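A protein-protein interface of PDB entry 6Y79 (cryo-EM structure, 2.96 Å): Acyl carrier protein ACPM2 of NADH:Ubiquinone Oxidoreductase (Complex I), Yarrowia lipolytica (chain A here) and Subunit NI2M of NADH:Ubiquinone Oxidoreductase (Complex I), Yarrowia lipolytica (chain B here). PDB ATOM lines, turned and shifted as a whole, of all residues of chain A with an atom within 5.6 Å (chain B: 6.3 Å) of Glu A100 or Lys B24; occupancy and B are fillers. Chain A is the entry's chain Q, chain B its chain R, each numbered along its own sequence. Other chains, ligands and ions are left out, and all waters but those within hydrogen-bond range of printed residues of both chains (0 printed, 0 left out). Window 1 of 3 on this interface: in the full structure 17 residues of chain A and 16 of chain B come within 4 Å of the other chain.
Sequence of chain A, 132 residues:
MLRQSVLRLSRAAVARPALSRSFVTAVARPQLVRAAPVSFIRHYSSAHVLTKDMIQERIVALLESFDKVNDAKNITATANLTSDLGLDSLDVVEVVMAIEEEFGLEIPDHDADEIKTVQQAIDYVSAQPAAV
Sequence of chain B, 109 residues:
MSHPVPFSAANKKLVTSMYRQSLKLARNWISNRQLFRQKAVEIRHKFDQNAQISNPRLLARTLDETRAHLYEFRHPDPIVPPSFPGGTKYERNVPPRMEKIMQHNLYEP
O of Ile A107 lies within hydrogen-bond range of NZ of Lys B24 (3.0 Å). The guanidinium group (NH2) of Arg B20 sits close to the backbone carbonyl oxygen (O) of Pro A108 (3.4 Å). O of Ile A107 sits close to NH2 of Arg B20, at 2.3 Å.
Among the printed residues, merely in contact across the chains: Met A97 with Leu B23 (3.8 Å), Met A97 with Lys B24 (3.8 Å) and Glu A100 with Lys B24 (3.3 Å).
Of chain B, only Lys B24 comes within 4 Å of Glu A100. Lys B24 touches just these residues of chain A: Met A97 (3.8 Å), Glu A100 (3.3 Å) and Ile A107 (3.0 Å). Of the printed residues of chain B, Pro A108 touches Arg B20. Printed residues of chain A within 4 Å of Arg B20: Ile A107 and Pro A108. Gln B21 touches none of the printed residues of chain A. The nearest residue of chain A that does not touch Lys B24 is Pro A108 (5.1 Å).
Of the 14 printed residues of chain A, 4 touch a printed residue of chain B. Hydrophobic or aromatic side chains of chain A within 4 Å of the printed part of chain B: Met A97 and Ile A107. Of the 12 printed residues of chain B, 3 touch a printed residue of chain A. Hydrophobic or aromatic side chains of chain B that line the printed part of chain A: Leu B23. Among the printed residues, 6 pairs touch across the chains. Among the printed residues, no Asp or Glu carboxylate lies within 4 Å of a Lys or Arg side-chain nitrogen of the other chain.
O of Glu A100 lies within hydrogen-bond range of N of Leu A105, at 3.0 Å. OE1 of Glu A100 sits at hydrogen-bond distance from N of Ile A107.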
ATOM      1  N   VAL A  95      12.074   3.375 -16.732  1.00  0.00           N
ATOM      2  CA  VAL A  95      11.652   4.376 -15.764  1.00  0.00           C
ATOM      3  C   VAL A  95      12.834   5.235 -15.292  1.00  0.00           C
ATOM      4  O   VAL A  95      12.618   6.373 -14.879  1.00  0.00           O
ATOM      5  CB  VAL A  95      10.887   3.703 -14.609  1.00  0.00           C
ATOM      6  CG1 VAL A  95      11.815   2.962 -13.781  1.00  0.00           C
ATOM      7  CG2 VAL A  95      10.114   4.714 -13.759  1.00  0.00           C
ATOM      8  N   VAL A  96      14.089   4.777 -15.398  1.00  0.00           N
ATOM      9  CA  VAL A  96      15.208   5.693 -15.138  1.00  0.00           C
ATOM     10  C   VAL A  96      15.296   6.760 -16.235  1.00  0.00           C
ATOM     11  O   VAL A  96      15.514   7.948 -15.956  1.00  0.00           O
ATOM     12  CB  VAL A  96      16.531   4.915 -14.953  1.00  0.00           C
ATOM     13  CG1 VAL A  96      17.731   5.819 -15.101  1.00  0.00           C
ATOM     14  CG2 VAL A  96      16.569   4.309 -13.564  1.00  0.00           C
ATOM     15  N   MET A  97      15.059   6.363 -17.488  1.00  0.00           N
ATOM     16  CA  MET A  97      14.984   7.325 -18.586  1.00  0.00           C
ATOM     17  C   MET A  97      13.825   8.302 -18.397  1.00  0.00           C
ATOM     18  O   MET A  97      13.973   9.515 -18.614  1.00  0.00           O
ATOM     19  CB  MET A  97      14.843   6.569 -19.904  1.00  0.00           C
ATOM     20  CG  MET A  97      14.707   7.438 -21.130  1.00  0.00           C
ATOM     21  SD  MET A  97      16.272   8.158 -21.630  1.00  0.00           S
ATOM     22  CE  MET A  97      15.764   9.029 -23.107  1.00  0.00           C
ATOM     23  N   ALA A  98      12.677   7.794 -17.945  1.00  0.00           N
ATOM     24  CA  ALA A  98      11.515   8.649 -17.723  1.00  0.00           C
ATOM     25  C   ALA A  98      11.731   9.608 -16.559  1.00  0.00           C
ATOM     26  O   ALA A  98      11.312  10.768 -16.620  1.00  0.00           O
ATOM     27  CB  ALA A  98      10.281   7.787 -17.483  1.00  0.00           C
ATOM     28  N   ILE A  99      12.391   9.150 -15.494  1.00  0.00           N
ATOM     29  CA  ILE A  99      12.595  10.018 -14.344  1.00  0.00           C
ATOM     30  C   ILE A  99      13.695  11.033 -14.628  1.00  0.00           C
ATOM     31  O   ILE A  99      13.687  12.133 -14.060  1.00  0.00           O
ATOM     32  CB  ILE A  99      12.870   9.184 -13.073  1.00  0.00           C
ATOM     33  CG1 ILE A  99      12.696  10.016 -11.813  1.00  0.00           C
ATOM     34  CG2 ILE A  99      14.270   8.612 -13.038  1.00  0.00           C
ATOM     35  CD1 ILE A  99      12.794   9.186 -10.579  1.00  0.00           C
ATOM     36  N   GLU A 100      14.631  10.725 -15.534  1.00  0.00           N
ATOM     37  CA  GLU A 100      15.637  11.735 -15.830  1.00  0.00           C
ATOM     38  C   GLU A 100      15.112  12.777 -16.811  1.00  0.00           C
ATOM     39  O   GLU A 100      15.485  13.945 -16.706  1.00  0.00           O
ATOM     40  CB  GLU A 100      16.937  11.089 -16.329  1.00  0.00           C
ATOM     41  CG  GLU A 100      16.940  10.564 -17.740  1.00  0.00           C
ATOM     42  CD  GLU A 100      18.196   9.795 -18.063  1.00  0.00           C
ATOM     43  OE1 GLU A 100      19.168   9.895 -17.290  1.00  0.00           O
ATOM     44  OE2 GLU A 100      18.206   9.075 -19.080  1.00  0.00           O
ATOM     45  N   GLU A 101      14.209  12.413 -17.730  1.00  0.00           N
ATOM     46  CA  GLU A 101      13.577  13.453 -18.545  1.00  0.00           C
ATOM     47  C   GLU A 101      12.540  14.227 -17.743  1.00  0.00           C
ATOM     48  O   GLU A 101      12.280  15.406 -18.030  1.00  0.00           O
ATOM     49  CB  GLU A 101      12.961  12.848 -19.811  1.00  0.00           C
ATOM     50  CG  GLU A 101      12.420  13.879 -20.828  1.00  0.00           C
ATOM     51  CD  GLU A 101      13.496  14.831 -21.376  1.00  0.00           C
ATOM     52  OE1 GLU A 101      14.682  14.439 -21.474  1.00  0.00           O
ATOM     53  OE2 GLU A 101      13.156  15.994 -21.691  1.00  0.00           O
ATOM     54  N   GLU A 102      11.961  13.583 -16.722  1.00  0.00           N
ATOM     55  CA  GLU A 102      10.943  14.223 -15.900  1.00  0.00           C
ATOM     56  C   GLU A 102      11.525  15.391 -15.109  1.00  0.00           C
ATOM     57  O   GLU A 102      10.957  16.486 -15.096  1.00  0.00           O
ATOM     58  CB  GLU A 102      10.342  13.194 -14.956  1.00  0.00           C
ATOM     59  CG  GLU A 102       9.303  13.712 -13.971  1.00  0.00           C
ATOM     60  CD  GLU A 102       8.197  14.501 -14.633  1.00  0.00           C
ATOM     61  OE1 GLU A 102       7.325  13.864 -15.255  1.00  0.00           O
ATOM     62  OE2 GLU A 102       8.171  15.742 -14.495  1.00  0.00           O
ATOM     63  N   PHE A 103      12.673  15.196 -14.474  1.00  0.00           N
ATOM     64  CA  PHE A 103      13.288  16.251 -13.679  1.00  0.00           C
ATOM     65  C   PHE A 103      14.194  17.158 -14.489  1.00  0.00           C
ATOM     66  O   PHE A 103      14.754  18.102 -13.928  1.00  0.00           O
ATOM     67  CB  PHE A 103      14.065  15.638 -12.515  1.00  0.00           C
ATOM     68  CG  PHE A 103      13.180  15.093 -11.460  1.00  0.00           C
ATOM     69  CD1 PHE A 103      12.428  15.947 -10.671  1.00  0.00           C
ATOM     70  CD2 PHE A 103      13.064  13.734 -11.278  1.00  0.00           C
ATOM     71  CE1 PHE A 103      11.600  15.455  -9.710  1.00  0.00           C
ATOM     72  CE2 PHE A 103      12.242  13.243 -10.311  1.00  0.00           C
ATOM     73  CZ  PHE A 103      11.506  14.109  -9.529  1.00  0.00           C
ATOM     74  N   GLY A 104      14.340  16.901 -15.785  1.00  0.00           N
ATOM     75  CA  GLY A 104      15.203  17.718 -16.613  1.00  0.00           C
ATOM     76  C   GLY A 104      16.670  17.567 -16.303  1.00  0.00           C
ATOM     77  O   GLY A 104      17.425  18.531 -16.432  1.00  0.00           O
ATOM     78  N   LEU A 105      17.096  16.383 -15.881  1.00  0.00           N
ATOM     79  CA  LEU A 105      18.477  16.166 -15.495  1.00  0.00           C
ATOM     80  C   LEU A 105      19.013  14.916 -16.179  1.00  0.00           C
ATOM     81  O   LEU A 105      18.270  14.164 -16.803  1.00  0.00           O
ATOM     82  CB  LEU A 105      18.619  16.108 -13.964  1.00  0.00           C
ATOM     83  CG  LEU A 105      17.860  15.198 -13.008  1.00  0.00           C
ATOM     84  CD1 LEU A 105      18.550  13.899 -12.878  1.00  0.00           C
ATOM     85  CD2 LEU A 105      17.813  15.860 -11.653  1.00  0.00           C
ATOM     86  N   GLU A 106      20.323  14.718 -16.124  1.00  0.00           N
ATOM     87  CA  GLU A 106      20.918  13.581 -16.813  1.00  0.00           C
ATOM     88  C   GLU A 106      21.846  12.779 -15.919  1.00  0.00           C
ATOM     89  O   GLU A 106      22.549  13.327 -15.065  1.00  0.00           O
ATOM     90  CB  GLU A 106      21.633  14.002 -18.093  1.00  0.00           C
ATOM     91  CG  GLU A 106      20.627  14.172 -19.200  1.00  0.00           C
ATOM     92  CD  GLU A 106      21.217  14.537 -20.514  1.00  0.00           C
ATOM     93  OE1 GLU A 106      22.459  14.609 -20.653  1.00  0.00           O
ATOM     94  OE2 GLU A 106      20.399  14.842 -21.394  1.00  0.00           O
ATOM     95  N   ILE A 107      21.834  11.471 -16.149  1.00  0.00           N
ATOM     96  CA  ILE A 107      22.379  10.484 -15.232  1.00  0.00           C
ATOM     97  C   ILE A 107      23.454   9.704 -15.972  1.00  0.00           C
ATOM     98  O   ILE A 107      23.217   9.270 -17.099  1.00  0.00           O
ATOM     99  CB  ILE A 107      21.292   9.529 -14.706  1.00  0.00           C
ATOM    100  CG1 ILE A 107      20.218  10.313 -13.980  1.00  0.00           C
ATOM    101  CG2 ILE A 107      21.858   8.569 -13.715  1.00  0.00           C
ATOM    102  CD1 ILE A 107      20.784  11.084 -12.859  1.00  0.00           C
ATOM    103  N   PRO A 108      24.643   9.532 -15.407  1.00  0.00           N
ATOM    104  CA  PRO A 108      25.602   8.584 -15.978  1.00  0.00           C
ATOM    105  C   PRO A 108      25.214   7.158 -15.617  1.00  0.00           C
ATOM    106  O   PRO A 108      24.391   6.921 -14.736  1.00  0.00           O
ATOM    107  CB  PRO A 108      26.925   8.983 -15.324  1.00  0.00           C
ATOM    108  CG  PRO A 108      26.515   9.545 -14.021  1.00  0.00           C
ATOM    109  CD  PRO A 108      25.194  10.236 -14.240  1.00  0.00           C
ATOM    110  N   TYR B  19      20.671  -0.280 -23.119  1.00  0.00           N
ATOM    111  CA  TYR B  19      19.297   0.168 -23.326  1.00  0.00           C
ATOM    112  C   TYR B  19      19.124   1.645 -22.975  1.00  0.00           C
ATOM    113  O   TYR B  19      18.399   2.363 -23.684  1.00  0.00           O
ATOM    114  CB  TYR B  19      18.344  -0.708 -22.512  1.00  0.00           C
ATOM    115  CG  TYR B  19      16.880  -0.401 -22.717  1.00  0.00           C
ATOM    116  CD1 TYR B  19      16.287  -0.513 -23.964  1.00  0.00           C
ATOM    117  CD2 TYR B  19      16.086  -0.030 -21.653  1.00  0.00           C
ATOM    118  CE1 TYR B  19      14.944  -0.239 -24.142  1.00  0.00           C
ATOM    119  CE2 TYR B  19      14.756   0.253 -21.818  1.00  0.00           C
ATOM    120  CZ  TYR B  19      14.186   0.141 -23.054  1.00  0.00           C
ATOM    121  OH  TYR B  19      12.850   0.424 -23.179  1.00  0.00           O
ATOM    122  N   ARG B  20      19.774   2.095 -21.882  1.00  0.00           N
ATOM    123  CA  ARG B  20      19.933   3.521 -21.578  1.00  0.00           C
ATOM    124  C   ARG B  20      20.445   4.289 -22.781  1.00  0.00           C
ATOM    125  O   ARG B  20      19.879   5.317 -23.170  1.00  0.00           O
ATOM    126  CB  ARG B  20      20.934   3.723 -20.438  1.00  0.00           C
ATOM    127  CG  ARG B  20      20.421   3.557 -19.059  1.00  0.00           C
ATOM    128  CD  ARG B  20      21.495   3.633 -18.033  1.00  0.00           C
ATOM    129  NE  ARG B  20      21.577   4.998 -17.557  1.00  0.00           N
ATOM    130  CZ  ARG B  20      22.476   5.874 -17.974  1.00  0.00           C
ATOM    131  NH1 ARG B  20      23.380   5.527 -18.877  1.00  0.00           N
ATOM    132  NH2 ARG B  20      22.465   7.095 -17.480  1.00  0.00           N
ATOM    133  N   GLN B  21      21.517   3.775 -23.386  1.00  0.00           N
ATOM    134  CA  GLN B  21      22.208   4.461 -24.469  1.00  0.00           C
ATOM    135  C   GLN B  21      21.331   4.562 -25.709  1.00  0.00           C
ATOM    136  O   GLN B  21      21.272   5.615 -26.349  1.00  0.00           O
ATOM    137  CB  GLN B  21      23.499   3.728 -24.809  1.00  0.00           C
ATOM    138  CG  GLN B  21      24.650   4.090 -23.922  1.00  0.00           C
ATOM    139  CD  GLN B  21      25.852   3.228 -24.194  1.00  0.00           C
ATOM    140  OE1 GLN B  21      25.921   2.548 -25.218  1.00  0.00           O
ATOM    141  NE2 GLN B  21      26.799   3.232 -23.275  1.00  0.00           N
ATOM    142  N   SER B  22      20.651   3.464 -26.086  1.00  0.00           N
ATOM    143  CA  SER B  22      19.832   3.512 -27.309  1.00  0.00           C
ATOM    144  C   SER B  22      18.560   4.321 -27.129  1.00  0.00           C
ATOM    145  O   SER B  22      18.069   4.924 -28.094  1.00  0.00           O
ATOM    146  CB  SER B  22      19.446   2.123 -27.815  1.00  0.00           C
ATOM    147  OG  SER B  22      18.768   2.224 -29.005  1.00  0.00           O
ATOM    148  N   LEU B  23      17.994   4.323 -25.912  1.00  0.00           N
ATOM    149  CA  LEU B  23      16.865   5.208 -25.642  1.00  0.00           C
ATOM    150  C   LEU B  23      17.276   6.672 -25.738  1.00  0.00           C
ATOM    151  O   LEU B  23      16.620   7.472 -26.426  1.00  0.00           O
ATOM    152  CB  LEU B  23      16.281   4.924 -24.267  1.00  0.00           C
ATOM    153  CG  LEU B  23      15.307   3.768 -24.040  1.00  0.00           C
ATOM    154  CD1 LEU B  23      14.735   3.843 -22.628  1.00  0.00           C
ATOM    155  CD2 LEU B  23      14.201   3.793 -25.072  1.00  0.00           C
ATOM    156  N   LYS B  24      18.384   7.030 -25.073  1.00  0.00           N
ATOM    157  CA  LYS B  24      18.895   8.399 -25.113  1.00  0.00           C
ATOM    158  C   LYS B  24      19.302   8.793 -26.519  1.00  0.00           C
ATOM    159  O   LYS B  24      19.161   9.955 -26.917  1.00  0.00           O
ATOM    160  CB  LYS B  24      20.110   8.532 -24.204  1.00  0.00           C
ATOM    161  CG  LYS B  24      19.831   8.781 -22.764  1.00  0.00           C
ATOM    162  CD  LYS B  24      21.168   8.907 -22.070  1.00  0.00           C
ATOM    163  CE  LYS B  24      21.085   8.598 -20.602  1.00  0.00           C
ATOM    164  NZ  LYS B  24      22.394   8.864 -19.966  1.00  0.00           N
ATOM    165  N   LEU B  25      19.833   7.836 -27.276  1.00  0.00           N
ATOM    166  CA  LEU B  25      20.330   8.142 -28.602  1.00  0.00           C
ATOM    167  C   LEU B  25      19.179   8.284 -29.579  1.00  0.00           C
ATOM    168  O   LEU B  25      19.224   9.127 -30.467  1.00  0.00           O
ATOM    169  CB  LEU B  25      21.313   7.064 -29.039  1.00  0.00           C
ATOM    170  CG  LEU B  25      22.099   7.247 -30.305  1.00  0.00           C
ATOM    171  CD1 LEU B  25      22.627   8.669 -30.428  1.00  0.00           C
ATOM    172  CD2 LEU B  25      23.255   6.273 -30.332  1.00  0.00           C
ATOM    173  N   ALA B  26      18.117   7.498 -29.410  1.00  0.00           N
ATOM    174  CA  ALA B  26      16.918   7.690 -30.214  1.00  0.00           C
ATOM    175  C   ALA B  26      16.185   8.968 -29.836  1.00  0.00           C
ATOM    176  O   ALA B  26      15.391   9.472 -30.634  1.00  0.00           O
ATOM    177  CB  ALA B  26      15.988   6.486 -30.056  1.00  0.00           C
ATOM    178  N   ARG B  27      16.419   9.480 -28.621  1.00  0.00           N
ATOM    179  CA  ARG B  27      15.720  10.673 -28.148  1.00  0.00           C
ATOM    180  C   ARG B  27      16.034  11.907 -28.989  1.00  0.00           C
ATOM    181  O   ARG B  27      15.133  12.700 -29.287  1.00  0.00           O
ATOM    182  CB  ARG B  27      16.060  10.914 -26.678  1.00  0.00           C
ATOM    183  CG  ARG B  27      15.601  12.240 -26.111  1.00  0.00           C
ATOM    184  CD  ARG B  27      14.093  12.346 -26.094  1.00  0.00           C
ATOM    185  NE  ARG B  27      13.661  13.692 -25.739  1.00  0.00           N
ATOM    186  CZ  ARG B  27      13.475  14.671 -26.618  1.00  0.00           C
ATOM    187  NH1 ARG B  27      13.684  14.451 -27.911  1.00  0.00           N
ATOM    188  NH2 ARG B  27      13.077  15.867 -26.208  1.00  0.00           N
ATOM    189  N   ASN B  28      17.287  12.082 -29.412  1.00  0.00           N
ATOM    190  CA  ASN B  28      17.636  13.311 -30.111  1.00  0.00           C
ATOM    191  C   ASN B  28      17.553  13.214 -31.631  1.00  0.00           C
ATOM    192  O   ASN B  28      17.708  14.237 -32.301  1.00  0.00           O
ATOM    193  CB  ASN B  28      19.027  13.807 -29.679  1.00  0.00           C
ATOM    194  CG  ASN B  28      20.107  12.759 -29.795  1.00  0.00           C
ATOM    195  OD1 ASN B  28      20.030  11.837 -30.595  1.00  0.00           O
ATOM    196  ND2 ASN B  28      21.137  12.903 -28.979  1.00  0.00           N
ATOM    197  N   TRP B  29      17.313  12.032 -32.198  1.00  0.00           N
ATOM    198  CA  TRP B  29      16.999  11.986 -33.623  1.00  0.00           C
ATOM    199  C   TRP B  29      15.591  12.500 -33.893  1.00  0.00           C
ATOM    200  O   TRP B  29      15.386  13.333 -34.778  1.00  0.00           O
ATOM    201  CB  TRP B  29      17.127  10.571 -34.178  1.00  0.00           C
ATOM    202  CG  TRP B  29      18.501  10.009 -34.264  1.00  0.00           C
ATOM    203  CD1 TRP B  29      19.039   9.077 -33.446  1.00  0.00           C
ATOM    204  CD2 TRP B  29      19.495  10.294 -35.252  1.00  0.00           C
ATOM    205  NE1 TRP B  29      20.316   8.778 -33.830  1.00  0.00           N
ATOM    206  CE2 TRP B  29      20.619   9.510 -34.944  1.00  0.00           C
ATOM    207  CE3 TRP B  29      19.547  11.142 -36.359  1.00  0.00           C
ATOM    208  CZ2 TRP B  29      21.780   9.545 -35.699  1.00  0.00           C
ATOM    209  CZ3 TRP B  29      20.706  11.181 -37.107  1.00  0.00           C
ATOM    210  CH2 TRP B  29      21.806  10.387 -36.774  1.00  0.00           C
ATOM    211  N   PHE B  36       8.529   9.231 -31.869  1.00  0.00           N
ATOM    212  CA  PHE B  36       9.570   8.770 -30.969  1.00  0.00           C
ATOM    213  C   PHE B  36       9.080   7.635 -30.093  1.00  0.00           C
ATOM    214  O   PHE B  36       9.822   6.689 -29.833  1.00  0.00           O
ATOM    215  CB  PHE B  36      10.079   9.903 -30.086  1.00  0.00           C
ATOM    216  CG  PHE B  36      11.064   9.439 -29.075  1.00  0.00           C
ATOM    217  CD1 PHE B  36      12.202   8.771 -29.485  1.00  0.00           C
ATOM    218  CD2 PHE B  36      10.846   9.625 -27.725  1.00  0.00           C
ATOM    219  CE1 PHE B  36      13.101   8.302 -28.571  1.00  0.00           C
ATOM    220  CE2 PHE B  36      11.755   9.169 -26.800  1.00  0.00           C
ATOM    221  CZ  PHE B  36      12.887   8.511 -27.224  1.00  0.00           C
